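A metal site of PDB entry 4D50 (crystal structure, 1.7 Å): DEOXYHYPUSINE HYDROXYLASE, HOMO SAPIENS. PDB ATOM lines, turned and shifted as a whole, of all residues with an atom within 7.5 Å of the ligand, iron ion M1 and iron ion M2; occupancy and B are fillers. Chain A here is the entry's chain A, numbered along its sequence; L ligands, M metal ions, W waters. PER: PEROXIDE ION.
The backbone NH (N) of Met 242 lies within hydrogen-bond range of the side-chain amide oxygen (OD1) of Asn 240 (2.8 Å). OG of Ser 277 is in hydrogen-bond range of ND1 of His 245 (2.7 Å). A ring nitrogen (ND1) of His 61 lies within hydrogen-bond range of the backbone carbonyl oxygen (O) of Leu 58. ND1 of His 94 is in hydrogen-bond range of OG1 of Thr 126. A ring nitrogen (ND1) of His 212 lies within hydrogen-bond range of the backbone carbonyl oxygen (O) of Leu 209 (2.7 Å).
Water W3 lies within hydrogen-bond range of the side-chain carboxylate (OE2) of Glu 95 (2.9 Å) and the side-chain carboxylate (OE1) of Glu 98 (3.1 Å).
Merely in contact with the ligand: Met 91 (3.8 Å) and Met 242 (3.3 Å). Of the 24 residues printed, 8 come within 4 Å of the ligand. The nearest printed residue that does not touch the ligand is Val 243 (5.8 Å).
Within 4 Å of iron ion M1: His 94, Glu 95 and His 212. The nearest printed residue that does not touch iron ion M1 is His 61 (4.2 Å).
Within 4 Å of iron ion M2: His 61, His 245 and Glu 246. The nearest printed residue that does not touch iron ion M2 is His 212 (4.2 Å).
Iron ion M1 is bound by OE1 of Glu 95, water W2, water W3, O1 of the ligand, NE2 of His 94 and NE2 of His 212.
Iron ion M2 is bound by OE1 of Glu 246 (2.1 Å), water W1 (2.2 Å), O2 of the ligand (2.2 Å), NE2 of His 245 (2.2 Å), NE2 of His 61 (2.3 Å) and water W2 (2.4 Å).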
ATOM      1  N   LEU A  58     -18.991  -4.628  -8.584  1.00  0.00           N
ATOM      2  CA  LEU A  58     -19.542  -4.633  -7.201  1.00  0.00           C
ATOM      3  C   LEU A  58     -18.807  -5.672  -6.337  1.00  0.00           C
ATOM      4  O   LEU A  58     -18.224  -5.326  -5.284  1.00  0.00           O
ATOM      5  CB  LEU A  58     -21.039  -4.921  -7.147  1.00  0.00           C
ATOM      6  CG  LEU A  58     -21.573  -4.898  -5.724  1.00  0.00           C
ATOM      7  CD1 LEU A  58     -21.522  -3.493  -5.134  1.00  0.00           C
ATOM      8  CD2 LEU A  58     -23.027  -5.361  -5.643  1.00  0.00           C
ATOM      9  N   HIS A  61     -14.836  -4.788  -5.913  1.00  0.00           N
ATOM     10  CA  HIS A  61     -14.556  -3.670  -5.027  1.00  0.00           C
ATOM     11  C   HIS A  61     -14.821  -4.037  -3.561  1.00  0.00           C
ATOM     12  O   HIS A  61     -14.084  -3.586  -2.672  1.00  0.00           O
ATOM     13  CB  HIS A  61     -15.244  -2.408  -5.531  1.00  0.00           C
ATOM     14  CG  HIS A  61     -16.425  -1.986  -4.716  1.00  0.00           C
ATOM     15  ND1 HIS A  61     -17.553  -2.767  -4.594  1.00  0.00           N
ATOM     16  CD2 HIS A  61     -16.612  -0.889  -3.941  1.00  0.00           C
ATOM     17  CE1 HIS A  61     -18.436  -2.107  -3.836  1.00  0.00           C
ATOM     18  NE2 HIS A  61     -17.859  -0.993  -3.394  1.00  0.00           N
ATOM     19  N   GLU A  62     -15.760  -4.954  -3.311  1.00  0.00           N
ATOM     20  CA  GLU A  62     -15.990  -5.463  -1.917  1.00  0.00           C
ATOM     21  C   GLU A  62     -14.765  -6.330  -1.454  1.00  0.00           C
ATOM     22  O   GLU A  62     -14.367  -6.359  -0.271  1.00  0.00           O
ATOM     23  CB  GLU A  62     -17.262  -6.266  -1.883  1.00  0.00           C
ATOM     24  CG  GLU A  62     -18.137  -6.109  -0.654  1.00  0.00           C
ATOM     25  CD  GLU A  62     -18.863  -4.771  -0.662  1.00  0.00           C
ATOM     26  OE1 GLU A  62     -19.519  -4.409  -1.661  1.00  0.00           O
ATOM     27  OE2 GLU A  62     -18.649  -4.031   0.310  1.00  0.00           O
ATOM     28  N   TYR A  65     -12.304  -3.834  -0.387  1.00  0.00           N
ATOM     29  CA  TYR A  65     -12.705  -3.269   0.882  1.00  0.00           C
ATOM     30  C   TYR A  65     -12.406  -4.189   2.064  1.00  0.00           C
ATOM     31  O   TYR A  65     -11.808  -3.806   3.057  1.00  0.00           O
ATOM     32  CB  TYR A  65     -14.198  -2.958   0.868  1.00  0.00           C
ATOM     33  CG  TYR A  65     -14.789  -2.475   2.155  1.00  0.00           C
ATOM     34  CD1 TYR A  65     -14.565  -1.195   2.625  1.00  0.00           C
ATOM     35  CD2 TYR A  65     -15.471  -3.369   2.992  1.00  0.00           C
ATOM     36  CE1 TYR A  65     -15.109  -0.757   3.842  1.00  0.00           C
ATOM     37  CE2 TYR A  65     -16.053  -2.949   4.165  1.00  0.00           C
ATOM     38  CZ  TYR A  65     -15.797  -1.680   4.631  1.00  0.00           C
ATOM     39  OH  TYR A  65     -16.391  -1.313   5.778  1.00  0.00           O
ATOM     40  N   PRO A  90     -12.905   2.202 -12.142  1.00  0.00           N
ATOM     41  CA  PRO A  90     -12.530   3.217 -11.131  1.00  0.00           C
ATOM     42  C   PRO A  90     -12.890   2.853  -9.659  1.00  0.00           C
ATOM     43  O   PRO A  90     -12.113   3.066  -8.722  1.00  0.00           O
ATOM     44  CB  PRO A  90     -13.325   4.462 -11.571  1.00  0.00           C
ATOM     45  CG  PRO A  90     -13.505   4.302 -13.035  1.00  0.00           C
ATOM     46  CD  PRO A  90     -13.612   2.830 -13.295  1.00  0.00           C
ATOM     47  N   MET A  91     -14.104   2.367  -9.495  1.00  0.00           N
ATOM     48  CA  MET A  91     -14.641   1.971  -8.200  1.00  0.00           C
ATOM     49  C   MET A  91     -13.764   0.873  -7.560  1.00  0.00           C
ATOM     50  O   MET A  91     -13.565   0.835  -6.330  1.00  0.00           O
ATOM     51  CB  MET A  91     -16.072   1.498  -8.451  1.00  0.00           C
ATOM     52  CG  MET A  91     -16.754   0.616  -7.464  1.00  0.00           C
ATOM     53  SD  MET A  91     -18.392   0.344  -8.197  1.00  0.00           S
ATOM     54  CE  MET A  91     -19.142  -0.507  -6.824  1.00  0.00           C
ATOM     55  N   VAL A  92     -13.243  -0.005  -8.410  1.00  0.00           N
ATOM     56  CA  VAL A  92     -12.462  -1.095  -7.943  1.00  0.00           C
ATOM     57  C   VAL A  92     -11.044  -0.563  -7.570  1.00  0.00           C
ATOM     58  O   VAL A  92     -10.484  -0.914  -6.524  1.00  0.00           O
ATOM     59  CB  VAL A  92     -12.392  -2.226  -8.980  1.00  0.00           C
ATOM     60  CG1 VAL A  92     -11.415  -3.242  -8.546  1.00  0.00           C
ATOM     61  CG2 VAL A  92     -13.778  -2.899  -9.090  1.00  0.00           C
ATOM     62  N   HIS A  94     -10.205   2.513  -6.890  1.00  0.00           N
ATOM     63  CA  HIS A  94     -10.349   3.408  -5.717  1.00  0.00           C
ATOM     64  C   HIS A  94     -10.332   2.552  -4.471  1.00  0.00           C
ATOM     65  O   HIS A  94      -9.551   2.836  -3.485  1.00  0.00           O
ATOM     66  CB  HIS A  94     -11.619   4.297  -5.776  1.00  0.00           C
ATOM     67  CG  HIS A  94     -12.442   4.206  -4.549  1.00  0.00           C
ATOM     68  ND1 HIS A  94     -12.091   4.786  -3.350  1.00  0.00           N
ATOM     69  CD2 HIS A  94     -13.616   3.569  -4.345  1.00  0.00           C
ATOM     70  CE1 HIS A  94     -13.005   4.481  -2.450  1.00  0.00           C
ATOM     71  NE2 HIS A  94     -13.940   3.749  -3.037  1.00  0.00           N
ATOM     72  N   GLU A  95     -11.123   1.499  -4.466  1.00  0.00           N
ATOM     73  CA  GLU A  95     -11.269   0.682  -3.278  1.00  0.00           C
ATOM     74  C   GLU A  95      -9.933   0.048  -2.854  1.00  0.00           C
ATOM     75  O   GLU A  95      -9.632  -0.107  -1.685  1.00  0.00           O
ATOM     76  CB  GLU A  95     -12.386  -0.389  -3.387  1.00  0.00           C
ATOM     77  CG  GLU A  95     -13.041  -0.720  -2.085  1.00  0.00           C
ATOM     78  CD  GLU A  95     -13.825   0.433  -1.491  1.00  0.00           C
ATOM     79  OE1 GLU A  95     -14.691   1.090  -2.189  1.00  0.00           O
ATOM     80  OE2 GLU A  95     -13.539   0.807  -0.315  1.00  0.00           O
ATOM     81  N   GLU A  98      -7.771   2.896  -1.262  1.00  0.00           N
ATOM     82  CA  GLU A  98      -8.256   3.045   0.124  1.00  0.00           C
ATOM     83  C   GLU A  98      -7.823   1.903   1.065  1.00  0.00           C
ATOM     84  O   GLU A  98      -7.465   2.141   2.191  1.00  0.00           O
ATOM     85  CB  GLU A  98      -9.808   3.187   0.192  1.00  0.00           C
ATOM     86  CG  GLU A  98     -10.309   3.416   1.622  1.00  0.00           C
ATOM     87  CD  GLU A  98     -11.794   3.677   1.736  1.00  0.00           C
ATOM     88  OE1 GLU A  98     -12.352   4.356   0.848  1.00  0.00           O
ATOM     89  OE2 GLU A  98     -12.346   3.280   2.777  1.00  0.00           O
ATOM     90  N   THR A 126      -8.749   9.255  -3.762  1.00  0.00           N
ATOM     91  CA  THR A 126      -8.616   8.173  -2.770  1.00  0.00           C
ATOM     92  C   THR A 126      -7.151   8.106  -2.265  1.00  0.00           C
ATOM     93  O   THR A 126      -6.937   8.001  -1.057  1.00  0.00           O
ATOM     94  CB  THR A 126      -8.895   6.812  -3.409  1.00  0.00           C
ATOM     95  OG1 THR A 126     -10.299   6.810  -3.771  1.00  0.00           O
ATOM     96  CG2 THR A 126      -8.554   5.682  -2.521  1.00  0.00           C
ATOM     97  N   LEU A 209     -16.410  10.713  -5.350  1.00  0.00           N
ATOM     98  CA  LEU A 209     -15.837   9.990  -4.184  1.00  0.00           C
ATOM     99  C   LEU A 209     -16.452  10.476  -2.895  1.00  0.00           C
ATOM    100  O   LEU A 209     -16.958   9.679  -2.074  1.00  0.00           O
ATOM    101  CB  LEU A 209     -14.320  10.156  -4.125  1.00  0.00           C
ATOM    102  CG  LEU A 209     -13.628   9.105  -3.290  1.00  0.00           C
ATOM    103  CD1 LEU A 209     -13.615   7.758  -3.939  1.00  0.00           C
ATOM    104  CD2 LEU A 209     -12.220   9.544  -2.944  1.00  0.00           C
ATOM    105  N   HIS A 212     -20.117   9.461  -2.442  1.00  0.00           N
ATOM    106  CA  HIS A 212     -20.228   8.051  -2.147  1.00  0.00           C
ATOM    107  C   HIS A 212     -19.927   7.777  -0.705  1.00  0.00           C
ATOM    108  O   HIS A 212     -20.572   6.946  -0.081  1.00  0.00           O
ATOM    109  CB  HIS A 212     -19.410   7.226  -3.186  1.00  0.00           C
ATOM    110  CG  HIS A 212     -18.276   6.404  -2.676  1.00  0.00           C
ATOM    111  ND1 HIS A 212     -17.079   6.954  -2.290  1.00  0.00           N
ATOM    112  CD2 HIS A 212     -18.073   5.064  -2.679  1.00  0.00           C
ATOM    113  CE1 HIS A 212     -16.274   6.009  -1.885  1.00  0.00           C
ATOM    114  NE2 HIS A 212     -16.821   4.850  -2.159  1.00  0.00           N
ATOM    115  N   GLU A 213     -18.893   8.432  -0.193  1.00  0.00           N
ATOM    116  CA  GLU A 213     -18.567   8.305   1.200  1.00  0.00           C
ATOM    117  C   GLU A 213     -19.703   8.734   2.095  1.00  0.00           C
ATOM    118  O   GLU A 213     -19.956   8.098   3.136  1.00  0.00           O
ATOM    119  CB  GLU A 213     -17.268   9.052   1.520  1.00  0.00           C
ATOM    120  CG  GLU A 213     -16.656   8.584   2.804  1.00  0.00           C
ATOM    121  CD  GLU A 213     -16.083   7.168   2.748  1.00  0.00           C
ATOM    122  OE1 GLU A 213     -15.476   6.785   1.728  1.00  0.00           O
ATOM    123  OE2 GLU A 213     -16.241   6.458   3.778  1.00  0.00           O
ATOM    124  N   TYR A 216     -22.051   5.927   2.259  1.00  0.00           N
ATOM    125  CA  TYR A 216     -21.565   4.874   3.141  1.00  0.00           C
ATOM    126  C   TYR A 216     -21.810   5.229   4.628  1.00  0.00           C
ATOM    127  O   TYR A 216     -22.370   4.426   5.391  1.00  0.00           O
ATOM    128  CB  TYR A 216     -20.066   4.620   2.832  1.00  0.00           C
ATOM    129  CG  TYR A 216     -19.304   3.739   3.812  1.00  0.00           C
ATOM    130  CD1 TYR A 216     -18.626   4.289   4.927  1.00  0.00           C
ATOM    131  CD2 TYR A 216     -19.195   2.352   3.601  1.00  0.00           C
ATOM    132  CE1 TYR A 216     -17.902   3.463   5.833  1.00  0.00           C
ATOM    133  CE2 TYR A 216     -18.462   1.553   4.476  1.00  0.00           C
ATOM    134  CZ  TYR A 216     -17.857   2.115   5.600  1.00  0.00           C
ATOM    135  OH  TYR A 216     -17.069   1.289   6.447  1.00  0.00           O
ATOM    136  N   ASN A 240     -23.625   9.558 -10.464  1.00  0.00           N
ATOM    137  CA  ASN A 240     -22.589   8.577 -10.702  1.00  0.00           C
ATOM    138  C   ASN A 240     -22.978   7.184 -10.150  1.00  0.00           C
ATOM    139  O   ASN A 240     -23.520   7.109  -9.067  1.00  0.00           O
ATOM    140  CB  ASN A 240     -21.337   9.135 -10.023  1.00  0.00           C
ATOM    141  CG  ASN A 240     -20.179   8.243 -10.192  1.00  0.00           C
ATOM    142  OD1 ASN A 240     -20.121   7.191  -9.633  1.00  0.00           O
ATOM    143  ND2 ASN A 240     -19.243   8.648 -11.004  1.00  0.00           N
ATOM    144  N   PRO A 241     -22.807   6.100 -10.938  1.00  0.00           N
ATOM    145  CA  PRO A 241     -23.223   4.782 -10.534  1.00  0.00           C
ATOM    146  C   PRO A 241     -22.578   4.316  -9.218  1.00  0.00           C
ATOM    147  O   PRO A 241     -23.242   3.643  -8.387  1.00  0.00           O
ATOM    148  CB  PRO A 241     -22.792   3.861 -11.678  1.00  0.00           C
ATOM    149  CG  PRO A 241     -22.332   4.756 -12.758  1.00  0.00           C
ATOM    150  CD  PRO A 241     -22.434   6.171 -12.370  1.00  0.00           C
ATOM    151  N   MET A 242     -21.355   4.747  -8.948  1.00  0.00           N
ATOM    152  CA  MET A 242     -20.694   4.417  -7.679  1.00  0.00           C
ATOM    153  C   MET A 242     -21.429   5.065  -6.491  1.00  0.00           C
ATOM    154  O   MET A 242     -21.536   4.460  -5.419  1.00  0.00           O
ATOM    155  CB  MET A 242     -19.235   4.898  -7.746  1.00  0.00           C
ATOM    156  CG  MET A 242     -18.446   4.771  -6.477  1.00  0.00           C
ATOM    157  SD  MET A 242     -16.759   5.357  -6.682  1.00  0.00           S
ATOM    158  CE  MET A 242     -17.150   7.102  -6.490  1.00  0.00           C
ATOM    159  N   VAL A 243     -21.924   6.286  -6.662  1.00  0.00           N
ATOM    160  CA  VAL A 243     -22.718   6.978  -5.631  1.00  0.00           C
ATOM    161  C   VAL A 243     -24.120   6.316  -5.482  1.00  0.00           C
ATOM    162  O   VAL A 243     -24.602   6.052  -4.347  1.00  0.00           O
ATOM    163  CB  VAL A 243     -22.981   8.455  -5.972  1.00  0.00           C
ATOM    164  CG1 VAL A 243     -23.853   9.095  -4.937  1.00  0.00           C
ATOM    165  CG2 VAL A 243     -21.611   9.223  -6.082  1.00  0.00           C
ATOM    166  N   HIS A 245     -24.941   3.265  -6.216  1.00  0.00           N
ATOM    167  CA  HIS A 245     -24.692   1.961  -5.513  1.00  0.00           C
ATOM    168  C   HIS A 245     -24.526   2.102  -4.003  1.00  0.00           C
ATOM    169  O   HIS A 245     -25.106   1.320  -3.224  1.00  0.00           O
ATOM    170  CB  HIS A 245     -23.526   1.198  -6.113  1.00  0.00           C
ATOM    171  CG  HIS A 245     -22.536   0.762  -5.106  1.00  0.00           C
ATOM    172  ND1 HIS A 245     -22.744  -0.358  -4.325  1.00  0.00           N
ATOM    173  CD2 HIS A 245     -21.300   1.215  -4.787  1.00  0.00           C
ATOM    174  CE1 HIS A 245     -21.727  -0.502  -3.505  1.00  0.00           C
ATOM    175  NE2 HIS A 245     -20.797   0.384  -3.818  1.00  0.00           N
ATOM    176  N   GLU A 246     -23.769   3.125  -3.541  1.00  0.00           N
ATOM    177  CA  GLU A 246     -23.531   3.280  -2.141  1.00  0.00           C
ATOM    178  C   GLU A 246     -24.823   3.652  -1.389  1.00  0.00           C
ATOM    179  O   GLU A 246     -25.059   3.156  -0.288  1.00  0.00           O
ATOM    180  CB  GLU A 246     -22.401   4.325  -1.926  1.00  0.00           C
ATOM    181  CG  GLU A 246     -21.532   4.030  -0.734  1.00  0.00           C
ATOM    182  CD  GLU A 246     -20.800   2.727  -0.856  1.00  0.00           C
ATOM    183  OE1 GLU A 246     -20.050   2.512  -1.811  1.00  0.00           O
ATOM    184  OE2 GLU A 246     -21.028   1.889   0.043  1.00  0.00           O
ATOM    185  N   GLU A 249     -26.890   0.498  -1.070  1.00  0.00           N
ATOM    186  CA  GLU A 249     -26.368  -0.259   0.060  1.00  0.00           C
ATOM    187  C   GLU A 249     -26.837   0.317   1.365  1.00  0.00           C
ATOM    188  O   GLU A 249     -27.202  -0.430   2.252  1.00  0.00           O
ATOM    189  CB  GLU A 249     -24.836  -0.301   0.071  1.00  0.00           C
ATOM    190  CG  GLU A 249     -24.194  -1.372  -0.764  1.00  0.00           C
ATOM    191  CD  GLU A 249     -22.890  -1.947  -0.137  1.00  0.00           C
ATOM    192  OE1 GLU A 249     -22.519  -1.744   1.039  1.00  0.00           O
ATOM    193  OE2 GLU A 249     -22.224  -2.644  -0.888  1.00  0.00           O
ATOM    194  N   VAL A 273     -23.881  -2.208 -11.506  1.00  0.00           N
ATOM    195  CA  VAL A 273     -23.471  -2.033 -10.121  1.00  0.00           C
ATOM    196  C   VAL A 273     -24.695  -1.665  -9.222  1.00  0.00           C
ATOM    197  O   VAL A 273     -24.831  -2.122  -8.070  1.00  0.00           O
ATOM    198  CB  VAL A 273     -22.356  -0.995  -9.983  1.00  0.00           C
ATOM    199  CG1 VAL A 273     -21.798  -1.029  -8.578  1.00  0.00           C
ATOM    200  CG2 VAL A 273     -21.233  -1.251 -10.992  1.00  0.00           C
ATOM    201  N   SER A 277     -26.379  -4.159  -6.353  1.00  0.00           N
ATOM    202  CA  SER A 277     -26.551  -3.661  -4.971  1.00  0.00           C
ATOM    203  C   SER A 277     -27.973  -3.851  -4.478  1.00  0.00           C
ATOM    204  O   SER A 277     -28.183  -4.297  -3.332  1.00  0.00           O
ATOM    205  CB  SER A 277     -26.119  -2.199  -4.730  1.00  0.00           C
ATOM    206  OG  SER A 277     -24.726  -2.166  -4.860  1.00  0.00           O
HETATM  207  O1  PER L   1     -16.937   2.228  -3.989  1.00  0.00           O
HETATM  208  O2  PER L   1     -18.445   2.219  -4.344  1.00  0.00           O
HETATM  209 FE    FE M   1     -15.794   2.832  -2.185  1.00  0.00          FE
HETATM  210 FE    FE M   2     -18.994   0.921  -2.675  1.00  0.00          FE
HETATM  211  O   HOH W   1     -19.651  -0.218  -0.960  1.00  0.00           O
HETATM  212  O   HOH W   2     -17.292   1.661  -1.195  1.00  0.00           O
HETATM  213  O   HOH W   3     -15.087   3.283  -0.173  1.00  0.00           O
